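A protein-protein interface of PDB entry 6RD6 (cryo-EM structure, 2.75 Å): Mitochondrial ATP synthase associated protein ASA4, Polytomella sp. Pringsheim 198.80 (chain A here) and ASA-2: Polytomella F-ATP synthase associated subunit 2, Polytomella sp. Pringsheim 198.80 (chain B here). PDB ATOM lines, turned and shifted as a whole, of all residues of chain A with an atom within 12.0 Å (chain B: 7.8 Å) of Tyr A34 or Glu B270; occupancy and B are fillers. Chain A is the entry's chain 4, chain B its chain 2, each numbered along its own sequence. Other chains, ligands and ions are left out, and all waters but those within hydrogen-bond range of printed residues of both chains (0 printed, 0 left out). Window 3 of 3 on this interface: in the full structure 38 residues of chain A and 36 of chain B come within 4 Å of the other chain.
O of Asp B274 sits at hydrogen-bond distance from NZ of Lys A27 (2.6 Å). The side-chain amino group of Lys B305 lies within hydrogen-bond range of the backbone carbonyl oxygen of Leu A33, 3.0 Å away. The side-chain amino group (NZ) of Lys B305 sits at hydrogen-bond distance from the backbone carbonyl oxygen (O) of Ala A37, at 2.7 Å.
The side-chain hydroxyl (OG) of Ser B301 lies within hydrogen-bond range of the backbone carbonyl oxygen (O) of Ala B298, 3.2 Å away. The backbone NH of Ala A37 is in hydrogen-bond range of the backbone carbonyl oxygen of Ser A32, at 3.3 Å.
Among the printed residues, pairs that only touch across the chains: Leu A30 with Phe B302 (3.2 Å), Tyr A34 with Glu B270 (3.4 Å), Tyr A34 with Pro B273 (3.6 Å), Tyr A34 with Phe B302 (3.7 Å), Lys A31 with Asp B274 (3.7 Å), Gly A36 with Lys B305 (3.8 Å), Tyr A34 with Val B299 (3.9 Å) and Tyr A34 with Ala B298 (3.99 Å).
Printed residues of chain B within 4 Å of Lys A27: Asp B274. Of the printed residues of chain B, Tyr A34 touches Glu B270, Pro B273, Ala B298, Val B299 and Phe B302. No residue of chain A comes within 4 Å of Ala B266. No residue of chain A comes within 4 Å of Pro B267. No residue of chain A comes within 4 Å of Ile B269. Glu B270 touches just one residue of chain A: Tyr A34 (3.4 Å). No residue of chain A comes within 4 Å of Ala B272. Of the printed residues of chain A, Pro B273 touches Tyr A34. Printed residues of chain A within 4 Å of Asp B274: Lys A27 and Lys A31. No residue of chain A comes within 4 Å of Pro B296. Val B299 touches just one residue of chain A: Tyr A34 (3.9 Å). Of the printed residues of chain A, Lys B305 touches Leu A33, Gly A36 and Ala A37. The nearest printed residue of chain B that does not touch Leu A33 is Phe B302 (4.2 Å).
Hydrophobic or aromatic side chains of chain A that line the printed part of chain B: Leu A30 and Tyr A34. Of the 21 printed residues of chain B, 7 touch a printed residue of chain A. Printed residues of chain B that touch a printed residue of chain A: Glu B270, Pro B273, Asp B274, Ala B298, Val B299, Phe B302 and Lys B305. Hydrophobic or aromatic side chains of chain B within 4 Å of the printed part of chain A: Pro B273, Val B299 and Phe B302. Among the printed residues, 11 pairs touch across the chains.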
ATOM      1  N   VAL A  11      -6.631  18.312  -6.160  1.00  0.00           N
ATOM      2  CA  VAL A  11      -5.248  18.783  -6.154  1.00  0.00           C
ATOM      3  C   VAL A  11      -4.968  19.626  -7.396  1.00  0.00           C
ATOM      4  O   VAL A  11      -4.193  20.587  -7.344  1.00  0.00           O
ATOM      5  CB  VAL A  11      -4.266  17.602  -5.996  1.00  0.00           C
ATOM      6  CG1 VAL A  11      -4.240  16.692  -7.212  1.00  0.00           C
ATOM      7  CG2 VAL A  11      -2.871  18.095  -5.667  1.00  0.00           C
ATOM      8  N   ALA A  25      -1.702  20.127   1.195  1.00  0.00           N
ATOM      9  CA  ALA A  25      -2.155  18.945   0.466  1.00  0.00           C
ATOM     10  C   ALA A  25      -1.421  18.798  -0.863  1.00  0.00           C
ATOM     11  O   ALA A  25      -1.030  17.687  -1.242  1.00  0.00           O
ATOM     12  CB  ALA A  25      -3.663  19.011   0.240  1.00  0.00           C
ATOM     13  N   VAL A  26      -1.200  19.914  -1.564  1.00  0.00           N
ATOM     14  CA  VAL A  26      -0.444  19.896  -2.815  1.00  0.00           C
ATOM     15  C   VAL A  26       1.008  19.499  -2.562  1.00  0.00           C
ATOM     16  O   VAL A  26       1.592  18.716  -3.322  1.00  0.00           O
ATOM     17  CB  VAL A  26      -0.564  21.268  -3.506  1.00  0.00           C
ATOM     18  CG1 VAL A  26       0.548  21.510  -4.514  1.00  0.00           C
ATOM     19  CG2 VAL A  26      -1.898  21.379  -4.184  1.00  0.00           C
ATOM     20  N   LYS A  27       1.591  19.982  -1.464  1.00  0.00           N
ATOM     21  CA  LYS A  27       2.985  19.679  -1.158  1.00  0.00           C
ATOM     22  C   LYS A  27       3.159  18.220  -0.748  1.00  0.00           C
ATOM     23  O   LYS A  27       4.148  17.577  -1.113  1.00  0.00           O
ATOM     24  CB  LYS A  27       3.484  20.620  -0.062  1.00  0.00           C
ATOM     25  CG  LYS A  27       3.856  22.009  -0.562  1.00  0.00           C
ATOM     26  CD  LYS A  27       4.158  22.944   0.593  1.00  0.00           C
ATOM     27  CE  LYS A  27       4.453  24.350   0.104  1.00  0.00           C
ATOM     28  NZ  LYS A  27       5.740  24.426  -0.635  1.00  0.00           N
ATOM     29  N   SER A  28       2.190  17.671  -0.009  1.00  0.00           N
ATOM     30  CA  SER A  28       2.249  16.257   0.341  1.00  0.00           C
ATOM     31  C   SER A  28       2.016  15.375  -0.880  1.00  0.00           C
ATOM     32  O   SER A  28       2.616  14.300  -0.998  1.00  0.00           O
ATOM     33  CB  SER A  28       1.233  15.941   1.435  1.00  0.00           C
ATOM     34  OG  SER A  28      -0.088  16.084   0.953  1.00  0.00           O
ATOM     35  N   TYR A  29       1.173  15.828  -1.814  1.00  0.00           N
ATOM     36  CA  TYR A  29       0.995  15.106  -3.071  1.00  0.00           C
ATOM     37  C   TYR A  29       2.269  15.119  -3.906  1.00  0.00           C
ATOM     38  O   TYR A  29       2.628  14.108  -4.519  1.00  0.00           O
ATOM     39  CB  TYR A  29      -0.164  15.715  -3.857  1.00  0.00           C
ATOM     40  CG  TYR A  29      -0.560  14.934  -5.084  1.00  0.00           C
ATOM     41  CD1 TYR A  29      -1.331  13.788  -4.975  1.00  0.00           C
ATOM     42  CD2 TYR A  29      -0.170  15.346  -6.350  1.00  0.00           C
ATOM     43  CE1 TYR A  29      -1.700  13.071  -6.090  1.00  0.00           C
ATOM     44  CE2 TYR A  29      -0.534  14.635  -7.473  1.00  0.00           C
ATOM     45  CZ  TYR A  29      -1.298  13.499  -7.335  1.00  0.00           C
ATOM     46  OH  TYR A  29      -1.667  12.782  -8.446  1.00  0.00           O
ATOM     47  N   LEU A  30       2.979  16.248  -3.919  1.00  0.00           N
ATOM     48  CA  LEU A  30       4.222  16.333  -4.678  1.00  0.00           C
ATOM     49  C   LEU A  30       5.325  15.503  -4.035  1.00  0.00           C
ATOM     50  O   LEU A  30       6.147  14.902  -4.735  1.00  0.00           O
ATOM     51  CB  LEU A  30       4.659  17.790  -4.808  1.00  0.00           C
ATOM     52  CG  LEU A  30       3.878  18.644  -5.803  1.00  0.00           C
ATOM     53  CD1 LEU A  30       4.467  20.040  -5.872  1.00  0.00           C
ATOM     54  CD2 LEU A  30       3.869  17.996  -7.171  1.00  0.00           C
ATOM     55  N   LYS A  31       5.351  15.445  -2.702  1.00  0.00           N
ATOM     56  CA  LYS A  31       6.307  14.577  -2.021  1.00  0.00           C
ATOM     57  C   LYS A  31       5.988  13.106  -2.265  1.00  0.00           C
ATOM     58  O   LYS A  31       6.898  12.279  -2.399  1.00  0.00           O
ATOM     59  CB  LYS A  31       6.323  14.889  -0.527  1.00  0.00           C
ATOM     60  CG  LYS A  31       7.319  15.967  -0.139  1.00  0.00           C
ATOM     61  CD  LYS A  31       6.805  16.835   0.997  1.00  0.00           C
ATOM     62  CE  LYS A  31       6.358  15.998   2.181  1.00  0.00           C
ATOM     63  NZ  LYS A  31       5.747  16.829   3.252  1.00  0.00           N
ATOM     64  N   SER A  32       4.697  12.769  -2.352  1.00  0.00           N
ATOM     65  CA  SER A  32       4.301  11.409  -2.697  1.00  0.00           C
ATOM     66  C   SER A  32       4.673  11.065  -4.135  1.00  0.00           C
ATOM     67  O   SER A  32       5.006   9.914  -4.435  1.00  0.00           O
ATOM     68  CB  SER A  32       2.799  11.233  -2.478  1.00  0.00           C
ATOM     69  OG  SER A  32       2.383   9.926  -2.820  1.00  0.00           O
ATOM     70  N   LEU A  33       4.613  12.044  -5.039  1.00  0.00           N
ATOM     71  CA  LEU A  33       5.021  11.790  -6.418  1.00  0.00           C
ATOM     72  C   LEU A  33       6.531  11.653  -6.533  1.00  0.00           C
ATOM     73  O   LEU A  33       7.029  10.872  -7.351  1.00  0.00           O
ATOM     74  CB  LEU A  33       4.530  12.901  -7.344  1.00  0.00           C
ATOM     75  CG  LEU A  33       3.043  13.013  -7.661  1.00  0.00           C
ATOM     76  CD1 LEU A  33       2.860  14.009  -8.780  1.00  0.00           C
ATOM     77  CD2 LEU A  33       2.453  11.672  -8.032  1.00  0.00           C
ATOM     78  N   TYR A  34       7.278  12.412  -5.731  1.00  0.00           N
ATOM     79  CA  TYR A  34       8.732  12.283  -5.738  1.00  0.00           C
ATOM     80  C   TYR A  34       9.171  10.990  -5.063  1.00  0.00           C
ATOM     81  O   TYR A  34      10.269  10.487  -5.323  1.00  0.00           O
ATOM     82  CB  TYR A  34       9.374  13.490  -5.057  1.00  0.00           C
ATOM     83  CG  TYR A  34      10.870  13.574  -5.251  1.00  0.00           C
ATOM     84  CD1 TYR A  34      11.743  13.144  -4.259  1.00  0.00           C
ATOM     85  CD2 TYR A  34      11.410  14.083  -6.424  1.00  0.00           C
ATOM     86  CE1 TYR A  34      13.105  13.215  -4.430  1.00  0.00           C
ATOM     87  CE2 TYR A  34      12.775  14.160  -6.603  1.00  0.00           C
ATOM     88  CZ  TYR A  34      13.617  13.725  -5.602  1.00  0.00           C
ATOM     89  OH  TYR A  34      14.974  13.797  -5.772  1.00  0.00           O
ATOM     90  N   ALA A  35       8.324  10.435  -4.190  1.00  0.00           N
ATOM     91  CA  ALA A  35       8.611   9.127  -3.611  1.00  0.00           C
ATOM     92  C   ALA A  35       8.498   8.021  -4.655  1.00  0.00           C
ATOM     93  O   ALA A  35       9.081   6.944  -4.495  1.00  0.00           O
ATOM     94  CB  ALA A  35       7.674   8.857  -2.436  1.00  0.00           C
ATOM     95  N   GLY A  36       7.748   8.264  -5.727  1.00  0.00           N
ATOM     96  CA  GLY A  36       7.690   7.338  -6.838  1.00  0.00           C
ATOM     97  C   GLY A  36       6.306   6.797  -7.123  1.00  0.00           C
ATOM     98  O   GLY A  36       6.164   5.759  -7.774  1.00  0.00           O
ATOM     99  N   ALA A  37       5.277   7.492  -6.650  1.00  0.00           N
ATOM    100  CA  ALA A  37       3.895   7.102  -6.885  1.00  0.00           C
ATOM    101  C   ALA A  37       3.474   7.577  -8.265  1.00  0.00           C
ATOM    102  O   ALA A  37       3.830   8.683  -8.679  1.00  0.00           O
ATOM    103  CB  ALA A  37       2.965   7.681  -5.819  1.00  0.00           C
ATOM    104  N   GLN A  38       2.731   6.737  -8.976  1.00  0.00           N
ATOM    105  CA  GLN A  38       2.267   7.103 -10.302  1.00  0.00           C
ATOM    106  C   GLN A  38       1.101   8.077 -10.204  1.00  0.00           C
ATOM    107  O   GLN A  38       0.239   7.954  -9.330  1.00  0.00           O
ATOM    108  CB  GLN A  38       1.851   5.857 -11.080  1.00  0.00           C
ATOM    109  CG  GLN A  38       3.021   5.051 -11.614  1.00  0.00           C
ATOM    110  CD  GLN A  38       3.736   5.756 -12.746  1.00  0.00           C
ATOM    111  OE1 GLN A  38       4.829   6.291 -12.568  1.00  0.00           O
ATOM    112  NE2 GLN A  38       3.118   5.764 -13.921  1.00  0.00           N
ATOM    113  N   VAL A  39       1.084   9.056 -11.102  1.00  0.00           N
ATOM    114  CA  VAL A  39      -0.007  10.021 -11.147  1.00  0.00           C
ATOM    115  C   VAL A  39      -1.231   9.350 -11.768  1.00  0.00           C
ATOM    116  O   VAL A  39      -1.129   8.644 -12.777  1.00  0.00           O
ATOM    117  CB  VAL A  39       0.415  11.303 -11.893  1.00  0.00           C
ATOM    118  CG1 VAL A  39       0.935  11.024 -13.299  1.00  0.00           C
ATOM    119  CG2 VAL A  39      -0.719  12.306 -11.935  1.00  0.00           C
ATOM    120  N   GLU A  40      -2.375   9.495 -11.106  1.00  0.00           N
ATOM    121  CA  GLU A  40      -3.613   8.884 -11.572  1.00  0.00           C
ATOM    122  C   GLU A  40      -4.062   9.545 -12.870  1.00  0.00           C
ATOM    123  O   GLU A  40      -3.917  10.757 -13.041  1.00  0.00           O
ATOM    124  CB  GLU A  40      -4.681   9.021 -10.483  1.00  0.00           C
ATOM    125  CG  GLU A  40      -6.086   8.593 -10.863  1.00  0.00           C
ATOM    126  CD  GLU A  40      -7.131   9.137  -9.909  1.00  0.00           C
ATOM    127  OE1 GLU A  40      -6.887   9.123  -8.685  1.00  0.00           O
ATOM    128  OE2 GLU A  40      -8.195   9.586 -10.385  1.00  0.00           O
ATOM    129  N   VAL B 265      19.455  23.872 -10.082  1.00  0.00           N
ATOM    130  CA  VAL B 265      18.069  23.693  -9.649  1.00  0.00           C
ATOM    131  C   VAL B 265      17.812  22.269  -9.142  1.00  0.00           C
ATOM    132  O   VAL B 265      16.990  22.062  -8.241  1.00  0.00           O
ATOM    133  CB  VAL B 265      17.098  24.110 -10.777  1.00  0.00           C
ATOM    134  CG1 VAL B 265      17.187  23.198 -11.977  1.00  0.00           C
ATOM    135  CG2 VAL B 265      15.677  24.187 -10.263  1.00  0.00           C
ATOM    136  N   ALA B 266      18.528  21.272  -9.668  1.00  0.00           N
ATOM    137  CA  ALA B 266      18.268  19.871  -9.353  1.00  0.00           C
ATOM    138  C   ALA B 266      18.569  19.436  -7.912  1.00  0.00           C
ATOM    139  O   ALA B 266      17.818  18.601  -7.394  1.00  0.00           O
ATOM    140  CB  ALA B 266      19.025  18.973 -10.338  1.00  0.00           C
ATOM    141  N   PRO B 267      19.616  19.926  -7.213  1.00  0.00           N
ATOM    142  CA  PRO B 267      19.697  19.597  -5.778  1.00  0.00           C
ATOM    143  C   PRO B 267      18.643  20.283  -4.926  1.00  0.00           C
ATOM    144  O   PRO B 267      18.362  19.816  -3.816  1.00  0.00           O
ATOM    145  CB  PRO B 267      21.112  20.048  -5.394  1.00  0.00           C
ATOM    146  CG  PRO B 267      21.860  20.024  -6.640  1.00  0.00           C
ATOM    147  CD  PRO B 267      20.899  20.509  -7.656  1.00  0.00           C
ATOM    148  N   ALA B 268      18.051  21.377  -5.411  1.00  0.00           N
ATOM    149  CA  ALA B 268      16.999  22.047  -4.653  1.00  0.00           C
ATOM    150  C   ALA B 268      15.724  21.213  -4.633  1.00  0.00           C
ATOM    151  O   ALA B 268      14.964  21.242  -3.661  1.00  0.00           O
ATOM    152  CB  ALA B 268      16.731  23.433  -5.237  1.00  0.00           C
ATOM    153  N   ILE B 269      15.478  20.456  -5.702  1.00  0.00           N
ATOM    154  CA  ILE B 269      14.330  19.557  -5.730  1.00  0.00           C
ATOM    155  C   ILE B 269      14.629  18.290  -4.937  1.00  0.00           C
ATOM    156  O   ILE B 269      13.731  17.682  -4.341  1.00  0.00           O
ATOM    157  CB  ILE B 269      13.940  19.255  -7.189  1.00  0.00           C
ATOM    158  CG1 ILE B 269      13.833  20.563  -7.967  1.00  0.00           C
ATOM    159  CG2 ILE B 269      12.620  18.507  -7.269  1.00  0.00           C
ATOM    160  CD1 ILE B 269      13.413  20.389  -9.388  1.00  0.00           C
ATOM    161  N   GLU B 270      15.900  17.884  -4.898  1.00  0.00           N
ATOM    162  CA  GLU B 270      16.282  16.718  -4.107  1.00  0.00           C
ATOM    163  C   GLU B 270      16.200  17.007  -2.613  1.00  0.00           C
ATOM    164  O   GLU B 270      15.844  16.124  -1.824  1.00  0.00           O
ATOM    165  CB  GLU B 270      17.687  16.261  -4.494  1.00  0.00           C
ATOM    166  CG  GLU B 270      17.774  15.674  -5.888  1.00  0.00           C
ATOM    167  CD  GLU B 270      19.181  15.247  -6.256  1.00  0.00           C
ATOM    168  OE1 GLU B 270      20.116  15.529  -5.479  1.00  0.00           O
ATOM    169  OE2 GLU B 270      19.350  14.628  -7.323  1.00  0.00           O
ATOM    170  N   LYS B 271      16.535  18.232  -2.202  1.00  0.00           N
ATOM    171  CA  LYS B 271      16.340  18.615  -0.807  1.00  0.00           C
ATOM    172  C   LYS B 271      14.862  18.792  -0.491  1.00  0.00           C
ATOM    173  O   LYS B 271      14.359  18.241   0.494  1.00  0.00           O
ATOM    174  CB  LYS B 271      17.111  19.898  -0.495  1.00  0.00           C
ATOM    175  CG  LYS B 271      18.620  19.736  -0.511  1.00  0.00           C
ATOM    176  CD  LYS B 271      19.318  21.039  -0.156  1.00  0.00           C
ATOM    177  CE  LYS B 271      20.826  20.906  -0.282  1.00  0.00           C
ATOM    178  NZ  LYS B 271      21.394  19.983   0.739  1.00  0.00           N
ATOM    179  N   ALA B 272      14.147  19.547  -1.321  1.00  0.00           N
ATOM    180  CA  ALA B 272      12.721  19.771  -1.127  1.00  0.00           C
ATOM    181  C   ALA B 272      12.006  19.735  -2.471  1.00  0.00           C
ATOM    182  O   ALA B 272      12.114  20.685  -3.256  1.00  0.00           O
ATOM    183  CB  ALA B 272      12.472  21.107  -0.428  1.00  0.00           C
ATOM    184  N   PRO B 273      11.271  18.660  -2.772  1.00  0.00           N
ATOM    185  CA  PRO B 273      10.534  18.596  -4.041  1.00  0.00           C
ATOM    186  C   PRO B 273       9.353  19.548  -4.057  1.00  0.00           C
ATOM    187  O   PRO B 273       8.941  20.046  -5.109  1.00  0.00           O
ATOM    188  CB  PRO B 273      10.068  17.136  -4.110  1.00  0.00           C
ATOM    189  CG  PRO B 273      10.795  16.422  -3.011  1.00  0.00           C
ATOM    190  CD  PRO B 273      11.097  17.439  -1.975  1.00  0.00           C
ATOM    191  N   ASP B 274       8.808  19.804  -2.874  1.00  0.00           N
ATOM    192  CA  ASP B 274       7.635  20.645  -2.704  1.00  0.00           C
ATOM    193  C   ASP B 274       7.968  22.126  -2.573  1.00  0.00           C
ATOM    194  O   ASP B 274       7.068  22.913  -2.265  1.00  0.00           O
ATOM    195  CB  ASP B 274       6.862  20.168  -1.479  1.00  0.00           C
ATOM    196  CG  ASP B 274       7.646  20.327  -0.193  1.00  0.00           C
ATOM    197  OD1 ASP B 274       8.889  20.232  -0.234  1.00  0.00           O
ATOM    198  OD2 ASP B 274       7.020  20.548   0.863  1.00  0.00           O
ATOM    199  N   LEU B 281       8.059  23.397 -12.060  1.00  0.00           N
ATOM    200  CA  LEU B 281       8.526  22.053 -12.384  1.00  0.00           C
ATOM    201  C   LEU B 281       8.120  21.654 -13.800  1.00  0.00           C
ATOM    202  O   LEU B 281       8.859  20.939 -14.489  1.00  0.00           O
ATOM    203  CB  LEU B 281       7.996  21.063 -11.356  1.00  0.00           C
ATOM    204  CG  LEU B 281       8.274  21.405  -9.896  1.00  0.00           C
ATOM    205  CD1 LEU B 281       7.242  20.759  -8.998  1.00  0.00           C
ATOM    206  CD2 LEU B 281       9.670  20.974  -9.505  1.00  0.00           C
ATOM    207  N   LEU B 295      18.748  15.245 -16.287  1.00  0.00           N
ATOM    208  CA  LEU B 295      18.501  15.549 -14.887  1.00  0.00           C
ATOM    209  C   LEU B 295      18.765  14.261 -14.119  1.00  0.00           C
ATOM    210  O   LEU B 295      19.013  13.224 -14.746  1.00  0.00           O
ATOM    211  CB  LEU B 295      17.065  16.040 -14.682  1.00  0.00           C
ATOM    212  CG  LEU B 295      16.687  17.444 -15.154  1.00  0.00           C
ATOM    213  CD1 LEU B 295      15.183  17.606 -15.125  1.00  0.00           C
ATOM    214  CD2 LEU B 295      17.350  18.502 -14.293  1.00  0.00           C
ATOM    215  N   PRO B 296      18.771  14.277 -12.786  1.00  0.00           N
ATOM    216  CA  PRO B 296      18.631  13.018 -12.044  1.00  0.00           C
ATOM    217  C   PRO B 296      17.317  12.325 -12.381  1.00  0.00           C
ATOM    218  O   PRO B 296      16.332  12.972 -12.743  1.00  0.00           O
ATOM    219  CB  PRO B 296      18.684  13.466 -10.583  1.00  0.00           C
ATOM    220  CG  PRO B 296      19.546  14.674 -10.614  1.00  0.00           C
ATOM    221  CD  PRO B 296      19.311  15.354 -11.934  1.00  0.00           C
ATOM    222  N   ALA B 297      17.318  10.994 -12.266  1.00  0.00           N
ATOM    223  CA  ALA B 297      16.208  10.178 -12.752  1.00  0.00           C
ATOM    224  C   ALA B 297      14.926  10.404 -11.959  1.00  0.00           C
ATOM    225  O   ALA B 297      13.831  10.484 -12.531  1.00  0.00           O
ATOM    226  CB  ALA B 297      16.603   8.701 -12.718  1.00  0.00           C
ATOM    227  N   ALA B 298      15.054  10.516 -10.633  1.00  0.00           N
ATOM    228  CA  ALA B 298      13.908  10.855  -9.799  1.00  0.00           C
ATOM    229  C   ALA B 298      13.413  12.262 -10.100  1.00  0.00           C
ATOM    230  O   ALA B 298      12.203  12.497 -10.181  1.00  0.00           O
ATOM    231  CB  ALA B 298      14.271  10.717  -8.322  1.00  0.00           C
ATOM    232  N   VAL B 299      14.342  13.196 -10.322  1.00  0.00           N
ATOM    233  CA  VAL B 299      13.981  14.569 -10.665  1.00  0.00           C
ATOM    234  C   VAL B 299      13.322  14.623 -12.041  1.00  0.00           C
ATOM    235  O   VAL B 299      12.333  15.338 -12.238  1.00  0.00           O
ATOM    236  CB  VAL B 299      15.225  15.475 -10.582  1.00  0.00           C
ATOM    237  CG1 VAL B 299      14.929  16.884 -11.065  1.00  0.00           C
ATOM    238  CG2 VAL B 299      15.743  15.511  -9.159  1.00  0.00           C
ATOM    239  N   GLY B 300      13.824  13.835 -12.995  1.00  0.00           N
ATOM    240  CA  GLY B 300      13.243  13.837 -14.332  1.00  0.00           C
ATOM    241  C   GLY B 300      11.848  13.239 -14.376  1.00  0.00           C
ATOM    242  O   GLY B 300      10.944  13.788 -15.015  1.00  0.00           O
ATOM    243  N   SER B 301      11.645  12.121 -13.668  1.00  0.00           N
ATOM    244  CA  SER B 301      10.308  11.543 -13.578  1.00  0.00           C
ATOM    245  C   SER B 301       9.360  12.454 -12.805  1.00  0.00           C
ATOM    246  O   SER B 301       8.173  12.561 -13.146  1.00  0.00           O
ATOM    247  CB  SER B 301      10.381  10.164 -12.928  1.00  0.00           C
ATOM    248  OG  SER B 301      10.341  10.265 -11.517  1.00  0.00           O
ATOM    249  N   PHE B 302       9.881  13.157 -11.794  1.00  0.00           N
ATOM    250  CA  PHE B 302       9.061  14.066 -11.006  1.00  0.00           C
ATOM    251  C   PHE B 302       8.621  15.275 -11.822  1.00  0.00           C
ATOM    252  O   PHE B 302       7.463  15.698 -11.736  1.00  0.00           O
ATOM    253  CB  PHE B 302       9.840  14.498  -9.766  1.00  0.00           C
ATOM    254  CG  PHE B 302       9.132  15.508  -8.926  1.00  0.00           C
ATOM    255  CD1 PHE B 302       9.635  16.790  -8.801  1.00  0.00           C
ATOM    256  CD2 PHE B 302       7.972  15.176  -8.251  1.00  0.00           C
ATOM    257  CE1 PHE B 302       8.992  17.723  -8.025  1.00  0.00           C
ATOM    258  CE2 PHE B 302       7.324  16.108  -7.473  1.00  0.00           C
ATOM    259  CZ  PHE B 302       7.836  17.383  -7.360  1.00  0.00           C
ATOM    260  N   VAL B 303       9.511  15.826 -12.649  1.00  0.00           N
ATOM    261  CA  VAL B 303       9.108  16.982 -13.444  1.00  0.00           C
ATOM    262  C   VAL B 303       8.247  16.549 -14.625  1.00  0.00           C
ATOM    263  O   VAL B 303       7.435  17.332 -15.121  1.00  0.00           O
ATOM    264  CB  VAL B 303      10.322  17.820 -13.891  1.00  0.00           C
ATOM    265  CG1 VAL B 303      11.083  18.342 -12.685  1.00  0.00           C
ATOM    266  CG2 VAL B 303      11.226  17.055 -14.829  1.00  0.00           C
ATOM    267  N   LYS B 305       5.888  14.118 -14.279  1.00  0.00           N
ATOM    268  CA  LYS B 305       4.585  14.032 -13.628  1.00  0.00           C
ATOM    269  C   LYS B 305       4.035  15.416 -13.300  1.00  0.00           C
ATOM    270  O   LYS B 305       2.822  15.650 -13.384  1.00  0.00           O
ATOM    271  CB  LYS B 305       4.691  13.180 -12.365  1.00  0.00           C
ATOM    272  CG  LYS B 305       4.995  11.724 -12.642  1.00  0.00           C
ATOM    273  CD  LYS B 305       4.895  10.882 -11.388  1.00  0.00           C
ATOM    274  CE  LYS B 305       6.232  10.259 -11.040  1.00  0.00           C
ATOM    275  NZ  LYS B 305       6.130   9.396  -9.838  1.00  0.00           N
